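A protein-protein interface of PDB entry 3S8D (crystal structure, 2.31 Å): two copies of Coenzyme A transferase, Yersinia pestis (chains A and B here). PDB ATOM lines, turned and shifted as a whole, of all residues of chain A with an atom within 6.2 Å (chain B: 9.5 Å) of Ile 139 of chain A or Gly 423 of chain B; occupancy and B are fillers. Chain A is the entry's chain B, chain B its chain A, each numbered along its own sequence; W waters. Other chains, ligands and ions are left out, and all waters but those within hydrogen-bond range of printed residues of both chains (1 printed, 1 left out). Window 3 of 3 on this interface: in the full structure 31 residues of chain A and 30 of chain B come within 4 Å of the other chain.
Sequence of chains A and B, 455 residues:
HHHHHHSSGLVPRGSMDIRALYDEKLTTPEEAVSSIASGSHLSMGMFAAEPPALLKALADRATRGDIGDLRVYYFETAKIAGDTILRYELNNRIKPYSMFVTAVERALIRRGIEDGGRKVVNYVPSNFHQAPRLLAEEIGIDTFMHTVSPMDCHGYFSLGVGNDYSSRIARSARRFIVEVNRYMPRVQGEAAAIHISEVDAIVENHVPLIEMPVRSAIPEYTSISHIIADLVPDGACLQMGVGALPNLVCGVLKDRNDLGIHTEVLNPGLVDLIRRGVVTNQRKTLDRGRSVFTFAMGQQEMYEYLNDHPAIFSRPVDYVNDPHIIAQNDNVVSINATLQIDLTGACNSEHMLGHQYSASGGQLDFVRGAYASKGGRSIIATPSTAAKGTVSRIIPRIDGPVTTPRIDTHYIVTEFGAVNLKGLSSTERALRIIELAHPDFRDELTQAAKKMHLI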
ATOM      1  N   HIS A  41     -27.256   8.506  24.211  1.00  0.00           N
ATOM      2  CA  HIS A  41     -27.154   7.588  23.084  1.00  0.00           C
ATOM      3  C   HIS A  41     -28.308   6.599  23.129  1.00  0.00           C
ATOM      4  O   HIS A  41     -28.548   5.926  24.150  1.00  0.00           O
ATOM      5  CB  HIS A  41     -25.839   6.807  23.132  1.00  0.00           C
ATOM      6  CG  HIS A  41     -24.621   7.660  23.020  1.00  0.00           C
ATOM      7  ND1 HIS A  41     -23.341   7.152  23.172  1.00  0.00           N
ATOM      8  CD2 HIS A  41     -24.470   8.983  22.778  1.00  0.00           C
ATOM      9  CE1 HIS A  41     -22.463   8.126  23.021  1.00  0.00           C
ATOM     10  NE2 HIS A  41     -23.125   9.248  22.778  1.00  0.00           N
ATOM     11  N   TYR A  73     -27.837   5.325  17.234  1.00  0.00           N
ATOM     12  CA  TYR A  73     -27.014   4.348  16.541  1.00  0.00           C
ATOM     13  C   TYR A  73     -27.889   3.167  16.150  1.00  0.00           C
ATOM     14  O   TYR A  73     -28.708   2.707  16.945  1.00  0.00           O
ATOM     15  CB  TYR A  73     -25.875   3.872  17.442  1.00  0.00           C
ATOM     16  CG  TYR A  73     -24.891   4.954  17.826  1.00  0.00           C
ATOM     17  CD1 TYR A  73     -23.708   5.124  17.121  1.00  0.00           C
ATOM     18  CD2 TYR A  73     -25.142   5.800  18.898  1.00  0.00           C
ATOM     19  CE1 TYR A  73     -22.805   6.108  17.469  1.00  0.00           C
ATOM     20  CE2 TYR A  73     -24.245   6.788  19.253  1.00  0.00           C
ATOM     21  CZ  TYR A  73     -23.077   6.937  18.535  1.00  0.00           C
ATOM     22  OH  TYR A  73     -22.179   7.917  18.882  1.00  0.00           O
ATOM     23  N   TYR A  97     -26.583   8.212  13.679  1.00  0.00           N
ATOM     24  CA  TYR A  97     -25.258   7.609  13.636  1.00  0.00           C
ATOM     25  C   TYR A  97     -25.489   6.231  13.091  1.00  0.00           C
ATOM     26  O   TYR A  97     -25.651   5.259  13.842  1.00  0.00           O
ATOM     27  CB  TYR A  97     -24.633   7.562  15.020  1.00  0.00           C
ATOM     28  CG  TYR A  97     -24.002   8.870  15.391  1.00  0.00           C
ATOM     29  CD1 TYR A  97     -22.625   9.001  15.442  1.00  0.00           C
ATOM     30  CD2 TYR A  97     -24.772   9.991  15.661  1.00  0.00           C
ATOM     31  CE1 TYR A  97     -22.025  10.204  15.763  1.00  0.00           C
ATOM     32  CE2 TYR A  97     -24.169  11.208  15.990  1.00  0.00           C
ATOM     33  CZ  TYR A  97     -22.796  11.303  16.038  1.00  0.00           C
ATOM     34  OH  TYR A  97     -22.167  12.490  16.352  1.00  0.00           O
ATOM     35  N   MET A  99     -24.597   2.939  11.084  1.00  0.00           N
ATOM     36  CA  MET A  99     -23.386   2.140  10.994  1.00  0.00           C
ATOM     37  C   MET A  99     -23.306   1.462   9.645  1.00  0.00           C
ATOM     38  O   MET A  99     -22.325   0.782   9.330  1.00  0.00           O
ATOM     39  CB  MET A  99     -23.304   1.140  12.151  1.00  0.00           C
ATOM     40  CG  MET A  99     -23.134   1.848  13.498  1.00  0.00           C
ATOM     41  SD  MET A  99     -23.559   0.815  14.927  1.00  0.00           S
ATOM     42  CE  MET A  99     -21.939   0.175  15.378  1.00  0.00           C
ATOM     43  N   VAL A 124     -20.838   5.752  10.961  1.00  0.00           N
ATOM     44  CA  VAL A 124     -19.938   5.111  11.920  1.00  0.00           C
ATOM     45  C   VAL A 124     -19.425   3.786  11.342  1.00  0.00           C
ATOM     46  O   VAL A 124     -20.070   2.742  11.473  1.00  0.00           O
ATOM     47  CB  VAL A 124     -20.643   4.849  13.265  1.00  0.00           C
ATOM     48  CG1 VAL A 124     -19.719   4.112  14.219  1.00  0.00           C
ATOM     49  CG2 VAL A 124     -21.131   6.144  13.882  1.00  0.00           C
ATOM     50  N   PRO A 125     -18.255   3.827  10.691  1.00  0.00           N
ATOM     51  CA  PRO A 125     -17.719   2.650   9.988  1.00  0.00           C
ATOM     52  C   PRO A 125     -17.463   1.504  10.959  1.00  0.00           C
ATOM     53  O   PRO A 125     -16.808   1.697  12.002  1.00  0.00           O
ATOM     54  CB  PRO A 125     -16.387   3.150   9.424  1.00  0.00           C
ATOM     55  CG  PRO A 125     -16.465   4.669   9.508  1.00  0.00           C
ATOM     56  CD  PRO A 125     -17.309   4.954  10.703  1.00  0.00           C
ATOM     57  N   ARG A 133     -20.212  -5.264  20.705  1.00  0.00           N
ATOM     58  CA  ARG A 133     -19.259  -4.664  21.612  1.00  0.00           C
ATOM     59  C   ARG A 133     -19.046  -3.174  21.309  1.00  0.00           C
ATOM     60  O   ARG A 133     -18.950  -2.369  22.233  1.00  0.00           O
ATOM     61  CB  ARG A 133     -17.951  -5.460  21.651  1.00  0.00           C
ATOM     62  CG  ARG A 133     -16.966  -5.169  20.546  1.00  0.00           C
ATOM     63  CD  ARG A 133     -15.656  -5.924  20.810  1.00  0.00           C
ATOM     64  NE  ARG A 133     -14.666  -5.141  21.561  1.00  0.00           N
ATOM     65  CZ  ARG A 133     -13.403  -5.533  21.747  1.00  0.00           C
ATOM     66  NH1 ARG A 133     -12.989  -6.690  21.236  1.00  0.00           N
ATOM     67  NH2 ARG A 133     -12.552  -4.765  22.426  1.00  0.00           N
ATOM     68  N   LEU A 134     -19.013  -2.813  20.026  1.00  0.00           N
ATOM     69  CA  LEU A 134     -18.916  -1.405  19.608  1.00  0.00           C
ATOM     70  C   LEU A 134     -19.983  -0.554  20.263  1.00  0.00           C
ATOM     71  O   LEU A 134     -19.716   0.530  20.771  1.00  0.00           O
ATOM     72  CB  LEU A 134     -19.057  -1.270  18.085  1.00  0.00           C
ATOM     73  CG  LEU A 134     -17.798  -1.580  17.267  1.00  0.00           C
ATOM     74  CD1 LEU A 134     -18.108  -1.633  15.757  1.00  0.00           C
ATOM     75  CD2 LEU A 134     -16.701  -0.559  17.572  1.00  0.00           C
ATOM     76  N   LEU A 135     -21.209  -1.043  20.222  1.00  0.00           N
ATOM     77  CA  LEU A 135     -22.300  -0.319  20.828  1.00  0.00           C
ATOM     78  C   LEU A 135     -22.192  -0.368  22.346  1.00  0.00           C
ATOM     79  O   LEU A 135     -22.375   0.650  23.005  1.00  0.00           O
ATOM     80  CB  LEU A 135     -23.637  -0.894  20.365  1.00  0.00           C
ATOM     81  CG  LEU A 135     -23.946  -0.571  18.902  1.00  0.00           C
ATOM     82  CD1 LEU A 135     -25.172  -1.330  18.402  1.00  0.00           C
ATOM     83  CD2 LEU A 135     -24.120   0.929  18.714  1.00  0.00           C
ATOM     84  N   ALA A 136     -21.878  -1.539  22.897  1.00  0.00           N
ATOM     85  CA  ALA A 136     -21.936  -1.713  24.343  1.00  0.00           C
ATOM     86  C   ALA A 136     -20.744  -1.083  25.053  1.00  0.00           C
ATOM     87  O   ALA A 136     -20.882  -0.548  26.155  1.00  0.00           O
ATOM     88  CB  ALA A 136     -22.058  -3.182  24.707  1.00  0.00           C
ATOM     89  N   GLU A 137     -19.577  -1.138  24.416  1.00  0.00           N
ATOM     90  CA  GLU A 137     -18.340  -0.733  25.079  1.00  0.00           C
ATOM     91  C   GLU A 137     -17.685   0.516  24.486  1.00  0.00           C
ATOM     92  O   GLU A 137     -17.254   1.415  25.221  1.00  0.00           O
ATOM     93  CB  GLU A 137     -17.343  -1.897  25.092  1.00  0.00           C
ATOM     94  CG  GLU A 137     -17.743  -3.038  26.050  1.00  0.00           C
ATOM     95  CD  GLU A 137     -17.016  -4.358  25.761  1.00  0.00           C
ATOM     96  OE1 GLU A 137     -15.749  -4.381  25.775  1.00  0.00           O
ATOM     97  OE2 GLU A 137     -17.733  -5.370  25.527  1.00  0.00           O
ATOM     98  N   GLU A 138     -17.586   0.579  23.165  1.00  0.00           N
ATOM     99  CA  GLU A 138     -16.842   1.680  22.568  1.00  0.00           C
ATOM    100  C   GLU A 138     -17.713   2.923  22.434  1.00  0.00           C
ATOM    101  O   GLU A 138     -17.220   4.038  22.483  1.00  0.00           O
ATOM    102  CB  GLU A 138     -16.274   1.281  21.208  1.00  0.00           C
ATOM    103  CG  GLU A 138     -15.657  -0.140  21.196  1.00  0.00           C
ATOM    104  CD  GLU A 138     -14.138  -0.126  21.356  1.00  0.00           C
ATOM    105  OE1 GLU A 138     -13.572   0.973  21.596  1.00  0.00           O
ATOM    106  OE2 GLU A 138     -13.515  -1.207  21.233  1.00  0.00           O
ATOM    107  N   ILE A 139     -19.013   2.731  22.270  1.00  0.00           N
ATOM    108  CA  ILE A 139     -19.921   3.860  22.132  1.00  0.00           C
ATOM    109  C   ILE A 139     -20.731   4.043  23.413  1.00  0.00           C
ATOM    110  O   ILE A 139     -20.731   5.122  24.014  1.00  0.00           O
ATOM    111  CB  ILE A 139     -20.836   3.671  20.920  1.00  0.00           C
ATOM    112  CG1 ILE A 139     -20.010   3.746  19.635  1.00  0.00           C
ATOM    113  CG2 ILE A 139     -21.935   4.730  20.894  1.00  0.00           C
ATOM    114  CD1 ILE A 139     -20.720   3.146  18.423  1.00  0.00           C
ATOM    115  N   GLY A 140     -21.389   2.979  23.856  1.00  0.00           N
ATOM    116  CA  GLY A 140     -22.182   3.060  25.069  1.00  0.00           C
ATOM    117  C   GLY A 140     -23.596   3.502  24.737  1.00  0.00           C
ATOM    118  O   GLY A 140     -23.794   4.584  24.182  1.00  0.00           O
ATOM    119  N   ILE A 141     -24.577   2.659  25.058  1.00  0.00           N
ATOM    120  CA  ILE A 141     -25.985   2.968  24.794  1.00  0.00           C
ATOM    121  C   ILE A 141     -26.752   3.179  26.079  1.00  0.00           C
ATOM    122  O   ILE A 141     -26.703   2.330  26.973  1.00  0.00           O
ATOM    123  CB  ILE A 141     -26.682   1.841  24.019  1.00  0.00           C
ATOM    124  CG1 ILE A 141     -25.945   1.587  22.705  1.00  0.00           C
ATOM    125  CG2 ILE A 141     -28.178   2.183  23.794  1.00  0.00           C
ATOM    126  CD1 ILE A 141     -25.798   2.827  21.795  1.00  0.00           C
ATOM    127  N   ARG A 174     -28.600   1.143  29.460  1.00  0.00           N
ATOM    128  CA  ARG A 174     -28.949   1.519  30.826  1.00  0.00           C
ATOM    129  C   ARG A 174     -30.463   1.496  31.090  1.00  0.00           C
ATOM    130  O   ARG A 174     -30.870   1.304  32.226  1.00  0.00           O
ATOM    131  CB  ARG A 174     -28.280   2.847  31.225  1.00  0.00           C
ATOM    132  CG  ARG A 174     -26.792   2.655  31.489  1.00  0.00           C
ATOM    133  CD  ARG A 174     -26.047   3.967  31.700  1.00  0.00           C
ATOM    134  NE  ARG A 174     -25.675   4.600  30.435  1.00  0.00           N
ATOM    135  CZ  ARG A 174     -24.625   4.229  29.703  1.00  0.00           C
ATOM    136  NH1 ARG A 174     -23.847   3.225  30.113  1.00  0.00           N
ATOM    137  NH2 ARG A 174     -24.353   4.862  28.557  1.00  0.00           N
ATOM    138  N   THR B 344     -10.044   8.638   7.016  1.00  0.00           N
ATOM    139  CA  THR B 344     -11.171   7.712   7.259  1.00  0.00           C
ATOM    140  C   THR B 344     -11.105   6.627   8.367  1.00  0.00           C
ATOM    141  O   THR B 344     -12.129   6.012   8.668  1.00  0.00           O
ATOM    142  CB  THR B 344     -11.692   7.036   5.958  1.00  0.00           C
ATOM    143  OG1 THR B 344     -10.591   6.472   5.236  1.00  0.00           O
ATOM    144  CG2 THR B 344     -12.424   8.047   5.075  1.00  0.00           C
ATOM    145  N   TYR B 371      -7.383  -6.878  18.301  1.00  0.00           N
ATOM    146  CA  TYR B 371      -8.615  -6.298  18.793  1.00  0.00           C
ATOM    147  C   TYR B 371      -9.534  -7.384  19.392  1.00  0.00           C
ATOM    148  O   TYR B 371     -10.187  -7.165  20.417  1.00  0.00           O
ATOM    149  CB  TYR B 371      -9.300  -5.488  17.676  1.00  0.00           C
ATOM    150  CG  TYR B 371     -10.540  -4.735  18.121  1.00  0.00           C
ATOM    151  CD1 TYR B 371     -10.443  -3.608  18.940  1.00  0.00           C
ATOM    152  CD2 TYR B 371     -11.818  -5.146  17.716  1.00  0.00           C
ATOM    153  CE1 TYR B 371     -11.594  -2.908  19.353  1.00  0.00           C
ATOM    154  CE2 TYR B 371     -12.963  -4.460  18.119  1.00  0.00           C
ATOM    155  CZ  TYR B 371     -12.846  -3.336  18.933  1.00  0.00           C
ATOM    156  OH  TYR B 371     -13.976  -2.639  19.337  1.00  0.00           O
ATOM    157  N   ARG B 406     -10.739   0.926   6.906  1.00  0.00           N
ATOM    158  CA  ARG B 406     -11.087   1.808   8.009  1.00  0.00           C
ATOM    159  C   ARG B 406     -11.872   1.094   9.110  1.00  0.00           C
ATOM    160  O   ARG B 406     -11.777   1.474  10.275  1.00  0.00           O
ATOM    161  CB  ARG B 406     -11.832   3.053   7.527  1.00  0.00           C
ATOM    162  CG  ARG B 406     -13.213   2.784   6.934  1.00  0.00           C
ATOM    163  CD  ARG B 406     -13.930   4.088   6.583  1.00  0.00           C
ATOM    164  NE  ARG B 406     -15.027   3.847   5.654  1.00  0.00           N
ATOM    165  CZ  ARG B 406     -15.773   4.799   5.091  1.00  0.00           C
ATOM    166  NH1 ARG B 406     -15.556   6.083   5.361  1.00  0.00           N
ATOM    167  NH2 ARG B 406     -16.751   4.462   4.252  1.00  0.00           N
ATOM    168  N   ILE B 407     -12.626   0.054   8.766  1.00  0.00           N
ATOM    169  CA  ILE B 407     -13.405  -0.640   9.792  1.00  0.00           C
ATOM    170  C   ILE B 407     -12.537  -1.534  10.693  1.00  0.00           C
ATOM    171  O   ILE B 407     -12.966  -1.941  11.777  1.00  0.00           O
ATOM    172  CB  ILE B 407     -14.530  -1.477   9.188  1.00  0.00           C
ATOM    173  CG1 ILE B 407     -13.976  -2.485   8.183  1.00  0.00           C
ATOM    174  CG2 ILE B 407     -15.567  -0.573   8.527  1.00  0.00           C
ATOM    175  CD1 ILE B 407     -15.040  -3.396   7.607  1.00  0.00           C
ATOM    176  N   ASP B 408     -11.317  -1.824  10.251  1.00  0.00           N
ATOM    177  CA  ASP B 408     -10.403  -2.659  11.027  1.00  0.00           C
ATOM    178  C   ASP B 408      -9.459  -1.869  11.926  1.00  0.00           C
ATOM    179  O   ASP B 408      -9.038  -2.350  12.965  1.00  0.00           O
ATOM    180  CB  ASP B 408      -9.582  -3.549  10.093  1.00  0.00           C
ATOM    181  CG  ASP B 408     -10.418  -4.624   9.450  1.00  0.00           C
ATOM    182  OD1 ASP B 408     -11.195  -5.285  10.183  1.00  0.00           O
ATOM    183  OD2 ASP B 408     -10.313  -4.792   8.215  1.00  0.00           O
ATOM    184  N   THR B 409      -9.106  -0.660  11.516  1.00  0.00           N
ATOM    185  CA  THR B 409      -8.168   0.138  12.305  1.00  0.00           C
ATOM    186  C   THR B 409      -8.638   0.286  13.757  1.00  0.00           C
ATOM    187  O   THR B 409      -9.810   0.578  14.021  1.00  0.00           O
ATOM    188  CB  THR B 409      -7.954   1.537  11.696  1.00  0.00           C
ATOM    189  OG1 THR B 409      -7.661   1.419  10.293  1.00  0.00           O
ATOM    190  CG2 THR B 409      -6.803   2.239  12.394  1.00  0.00           C
ATOM    191  N   HIS B 410      -7.710   0.070  14.683  1.00  0.00           N
ATOM    192  CA  HIS B 410      -7.955   0.255  16.106  1.00  0.00           C
ATOM    193  C   HIS B 410      -7.263   1.560  16.527  1.00  0.00           C
ATOM    194  O   HIS B 410      -7.839   2.651  16.422  1.00  0.00           O
ATOM    195  CB  HIS B 410      -7.358  -0.940  16.860  1.00  0.00           C
ATOM    196  CG  HIS B 410      -7.798  -1.037  18.299  1.00  0.00           C
ATOM    197  ND1 HIS B 410      -7.175  -1.896  19.189  1.00  0.00           N
ATOM    198  CD2 HIS B 410      -8.779  -0.425  18.976  1.00  0.00           C
ATOM    199  CE1 HIS B 410      -7.772  -1.791  20.369  1.00  0.00           C
ATOM    200  NE2 HIS B 410      -8.737  -0.904  20.277  1.00  0.00           N
ATOM    201  N   VAL B 419      -4.753   7.630  18.767  1.00  0.00           N
ATOM    202  CA  VAL B 419      -6.200   7.671  18.876  1.00  0.00           C
ATOM    203  C   VAL B 419      -6.802   6.330  18.504  1.00  0.00           C
ATOM    204  O   VAL B 419      -6.344   5.653  17.567  1.00  0.00           O
ATOM    205  CB  VAL B 419      -6.823   8.837  18.041  1.00  0.00           C
ATOM    206  CG1 VAL B 419      -6.447   8.717  16.573  1.00  0.00           C
ATOM    207  CG2 VAL B 419      -8.339   8.893  18.228  1.00  0.00           C
ATOM    208  N   ASN B 420      -7.811   5.941  19.273  1.00  0.00           N
ATOM    209  CA  ASN B 420      -8.589   4.738  19.001  1.00  0.00           C
ATOM    210  C   ASN B 420      -9.771   5.048  18.076  1.00  0.00           C
ATOM    211  O   ASN B 420     -10.736   5.706  18.485  1.00  0.00           O
ATOM    212  CB  ASN B 420      -9.116   4.161  20.316  1.00  0.00           C
ATOM    213  CG  ASN B 420      -9.954   2.897  20.110  1.00  0.00           C
ATOM    214  OD1 ASN B 420     -10.343   2.557  18.986  1.00  0.00           O
ATOM    215  ND2 ASN B 420     -10.256   2.217  21.203  1.00  0.00           N
ATOM    216  N   LEU B 421      -9.720   4.555  16.843  1.00  0.00           N
ATOM    217  CA  LEU B 421     -10.787   4.864  15.892  1.00  0.00           C
ATOM    218  C   LEU B 421     -12.109   4.128  16.137  1.00  0.00           C
ATOM    219  O   LEU B 421     -13.162   4.552  15.634  1.00  0.00           O
ATOM    220  CB  LEU B 421     -10.314   4.608  14.461  1.00  0.00           C
ATOM    221  CG  LEU B 421      -9.099   5.419  14.010  1.00  0.00           C
ATOM    222  CD1 LEU B 421      -8.823   5.155  12.538  1.00  0.00           C
ATOM    223  CD2 LEU B 421      -9.314   6.916  14.270  1.00  0.00           C
ATOM    224  N   LYS B 422     -12.065   3.030  16.886  1.00  0.00           N
ATOM    225  CA  LYS B 422     -13.246   2.149  16.958  1.00  0.00           C
ATOM    226  C   LYS B 422     -14.473   2.852  17.539  1.00  0.00           C
ATOM    227  O   LYS B 422     -14.443   3.313  18.674  1.00  0.00           O
ATOM    228  CB  LYS B 422     -12.938   0.875  17.755  1.00  0.00           C
ATOM    229  CG  LYS B 422     -11.983  -0.084  17.047  1.00  0.00           C
ATOM    230  CD  LYS B 422     -12.723  -0.889  15.988  1.00  0.00           C
ATOM    231  CE  LYS B 422     -11.775  -1.765  15.178  1.00  0.00           C
ATOM    232  NZ  LYS B 422     -12.531  -2.807  14.414  1.00  0.00           N
ATOM    233  N   GLY B 423     -15.551   2.944  16.758  1.00  0.00           N
ATOM    234  CA  GLY B 423     -16.782   3.535  17.257  1.00  0.00           C
ATOM    235  C   GLY B 423     -16.919   5.006  16.910  1.00  0.00           C
ATOM    236  O   GLY B 423     -17.999   5.600  17.047  1.00  0.00           O
ATOM    237  N   LEU B 424     -15.821   5.600  16.451  1.00  0.00           N
ATOM    238  CA  LEU B 424     -15.864   6.986  15.986  1.00  0.00           C
ATOM    239  C   LEU B 424     -16.621   7.123  14.666  1.00  0.00           C
ATOM    240  O   LEU B 424     -16.554   6.236  13.795  1.00  0.00           O
ATOM    241  CB  LEU B 424     -14.453   7.550  15.848  1.00  0.00           C
ATOM    242  CG  LEU B 424     -13.667   7.498  17.150  1.00  0.00           C
ATOM    243  CD1 LEU B 424     -12.392   8.322  17.039  1.00  0.00           C
ATOM    244  CD2 LEU B 424     -14.545   7.976  18.315  1.00  0.00           C
ATOM    245  N   SER B 425     -17.338   8.236  14.530  1.00  0.00           N
ATOM    246  CA  SER B 425     -18.013   8.591  13.285  1.00  0.00           C
ATOM    247  C   SER B 425     -17.009   9.116  12.254  1.00  0.00           C
ATOM    248  O   SER B 425     -15.861   9.427  12.590  1.00  0.00           O
ATOM    249  CB  SER B 425     -19.052   9.677  13.553  1.00  0.00           C
ATOM    250  OG  SER B 425     -18.425  10.914  13.859  1.00  0.00           O
ATOM    251  N   SER B 426     -17.434   9.221  11.000  1.00  0.00           N
ATOM    252  CA  SER B 426     -16.545   9.720   9.962  1.00  0.00           C
ATOM    253  C   SER B 426     -16.002  11.096  10.354  1.00  0.00           C
ATOM    254  O   SER B 426     -14.852  11.448  10.053  1.00  0.00           O
ATOM    255  CB  SER B 426     -17.270   9.768   8.619  1.00  0.00           C
ATOM    256  OG  SER B 426     -17.096   8.545   7.926  1.00  0.00           O
ATOM    257  N   THR B 427     -16.836  11.854  11.052  1.00  0.00           N
ATOM    258  CA  THR B 427     -16.479  13.182  11.510  1.00  0.00           C
ATOM    259  C   THR B 427     -15.462  13.111  12.636  1.00  0.00           C
ATOM    260  O   THR B 427     -14.362  13.671  12.522  1.00  0.00           O
ATOM    261  CB  THR B 427     -17.736  13.956  11.958  1.00  0.00           C
ATOM    262  OG1 THR B 427     -18.216  14.736  10.864  1.00  0.00           O
ATOM    263  CG2 THR B 427     -17.431  14.902  13.113  1.00  0.00           C
ATOM    264  N   GLU B 428     -15.830  12.430  13.720  1.00  0.00           N
ATOM    265  CA  GLU B 428     -14.926  12.226  14.851  1.00  0.00           C
ATOM    266  C   GLU B 428     -13.593  11.689  14.343  1.00  0.00           C
ATOM    267  O   GLU B 428     -12.519  12.164  14.727  1.00  0.00           O
ATOM    268  CB  GLU B 428     -15.547  11.264  15.874  1.00  0.00           C
ATOM    269  CG  GLU B 428     -16.776  11.818  16.644  1.00  0.00           C
ATOM    270  CD  GLU B 428     -17.575  10.713  17.382  1.00  0.00           C
ATOM    271  OE1 GLU B 428     -17.934  10.907  18.570  1.00  0.00           O
ATOM    272  OE2 GLU B 428     -17.865   9.656  16.764  1.00  0.00           O
ATOM    273  N   ARG B 429     -13.664  10.706  13.453  1.00  0.00           N
ATOM    274  CA  ARG B 429     -12.450  10.126  12.886  1.00  0.00           C
ATOM    275  C   ARG B 429     -11.558  11.140  12.130  1.00  0.00           C
ATOM    276  O   ARG B 429     -10.333  11.178  12.360  1.00  0.00           O
ATOM    277  CB  ARG B 429     -12.783   8.900  12.032  1.00  0.00           C
ATOM    278  CG  ARG B 429     -13.286   7.707  12.856  1.00  0.00           C
ATOM    279  CD  ARG B 429     -13.946   6.628  11.989  1.00  0.00           C
ATOM    280  NE  ARG B 429     -12.963   5.772  11.341  1.00  0.00           N
ATOM    281  CZ  ARG B 429     -12.724   4.509  11.676  1.00  0.00           C
ATOM    282  NH1 ARG B 429     -13.394   3.927  12.663  1.00  0.00           N
ATOM    283  NH2 ARG B 429     -11.805   3.831  11.011  1.00  0.00           N
HETATM  284  O   HOH W   1      -9.226  -5.689  22.242  1.00  0.00           O
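The side-chain hydroxyl (OH) of Tyr 371 of chain B sits at hydrogen-bond distance from the side-chain carboxylate (OE2) of Glu 138 of chain A (2.4 Å). O of Tyr 371 of chain B lies within hydrogen-bond range of NH1 of Arg 133 of chain A (3.0 Å).
N of Ser 425 of chain B sits at hydrogen-bond distance from OE2 of Glu 428 of chain B (2.7 Å). OD1 of Asn 420 of chain B lies within hydrogen-bond range of N of Lys 422 of chain B, 2.8 Å away. The backbone carbonyl oxygen (O) of Leu 421 of chain B lies within hydrogen-bond range of the guanidinium group (NH1) of Arg 429 of chain B, 3.0 Å away. The backbone carbonyl oxygen (O) of Ile 139 of chain A lies within hydrogen-bond range of a ring nitrogen (ND1) of His 41 of chain A, at 3.4 Å. The backbone carbonyl oxygen (O) of Thr 344 of chain B lies within hydrogen-bond range of the guanidinium group (NE) of Arg 429 of chain B (2.8 Å). The guanidinium group (NH2) of Arg 133 of chain A is in salt-bridge range of the side-chain carboxylate (OE2) of Glu 138 of chain A (3.9 Å).
Among the printed residues, pairs that only touch across the chains: Pro 125 of chain A with Leu 424 of chain B (3.4 Å), Glu 138 of chain A with Asn 420 of chain B (3.6 Å), Val 124 of chain A with Gly 423 of chain B (3.6 Å), Pro 125 of chain A with Ile 407 of chain B (3.7 Å), Glu 138 of chain A with Lys 422 of chain B (3.7 Å), Tyr 97 of chain A with Ser 425 of chain B (3.7 Å), Ile 139 of chain A with Gly 423 of chain B (3.8 Å), Leu 134 of chain A with Gly 423 of chain B (3.8 Å), Val 124 of chain A with Leu 424 of chain B (3.8 Å), Leu 134 of chain A with Tyr 371 of chain B (3.9 Å), Pro 125 of chain A with Arg 406 of chain B (3.9 Å) and Pro 125 of chain A with Arg 429 of chain B (3.97 Å).
Of chain B, only Gly 423 comes within 4 Å of Ile 139 of chain A. Gly 140 of chain A touches none of the printed residues of chain B. Printed residues of chain A within 4 Å of Tyr 371 of chain B: Arg 133 (3.0 Å), Leu 134 (3.9 Å) and Glu 138 (2.4 Å). Of chain A, only Val 124 (3.6 Å), Leu 134 (3.8 Å) and Ile 139 (3.8 Å) come within 4 Å of Gly 423 of chain B. Of the printed residues of chain A, Leu 424 of chain B touches Val 124 and Pro 125. Of the printed residues of chain A, Ser 425 of chain B touches Tyr 97 (3.7 Å). Thr 427 of chain B touches none of the printed residues of chain A. Glu 428 of chain B touches none of the printed residues of chain A. The nearest residue of chain A that does not touch Gly 423 of chain B is Glu 138 of chain A (4.6 Å). The nearest printed residue of chain B that does not touch Pro 125 of chain A is Ser 426 of chain B (4.2 Å).
Of the 18 printed residues of chain B, 9 touch a printed residue of chain A. Hydrophobic or aromatic side chains of chain B that line the printed part of chain A: Tyr 371 and Ile 407. Hydrophobic or aromatic side chains of chain A that line the printed part of chain B: Tyr 97, Val 124, Pro 125, Leu 134 and Ile 139. Among the printed residues, no Asp or Glu carboxylate lies within 4 Å of a Lys or Arg side-chain nitrogen of the other chain.
No position is printed for both chains. Of the 14 pairs that touch across the chains among the printed residues, none has its exchanged pair printed and touching as well.
Water W1 bridges O of Tyr 371 of chain B (2.5 Å) and NH2 of Arg 133 of chain A (3.5 Å).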
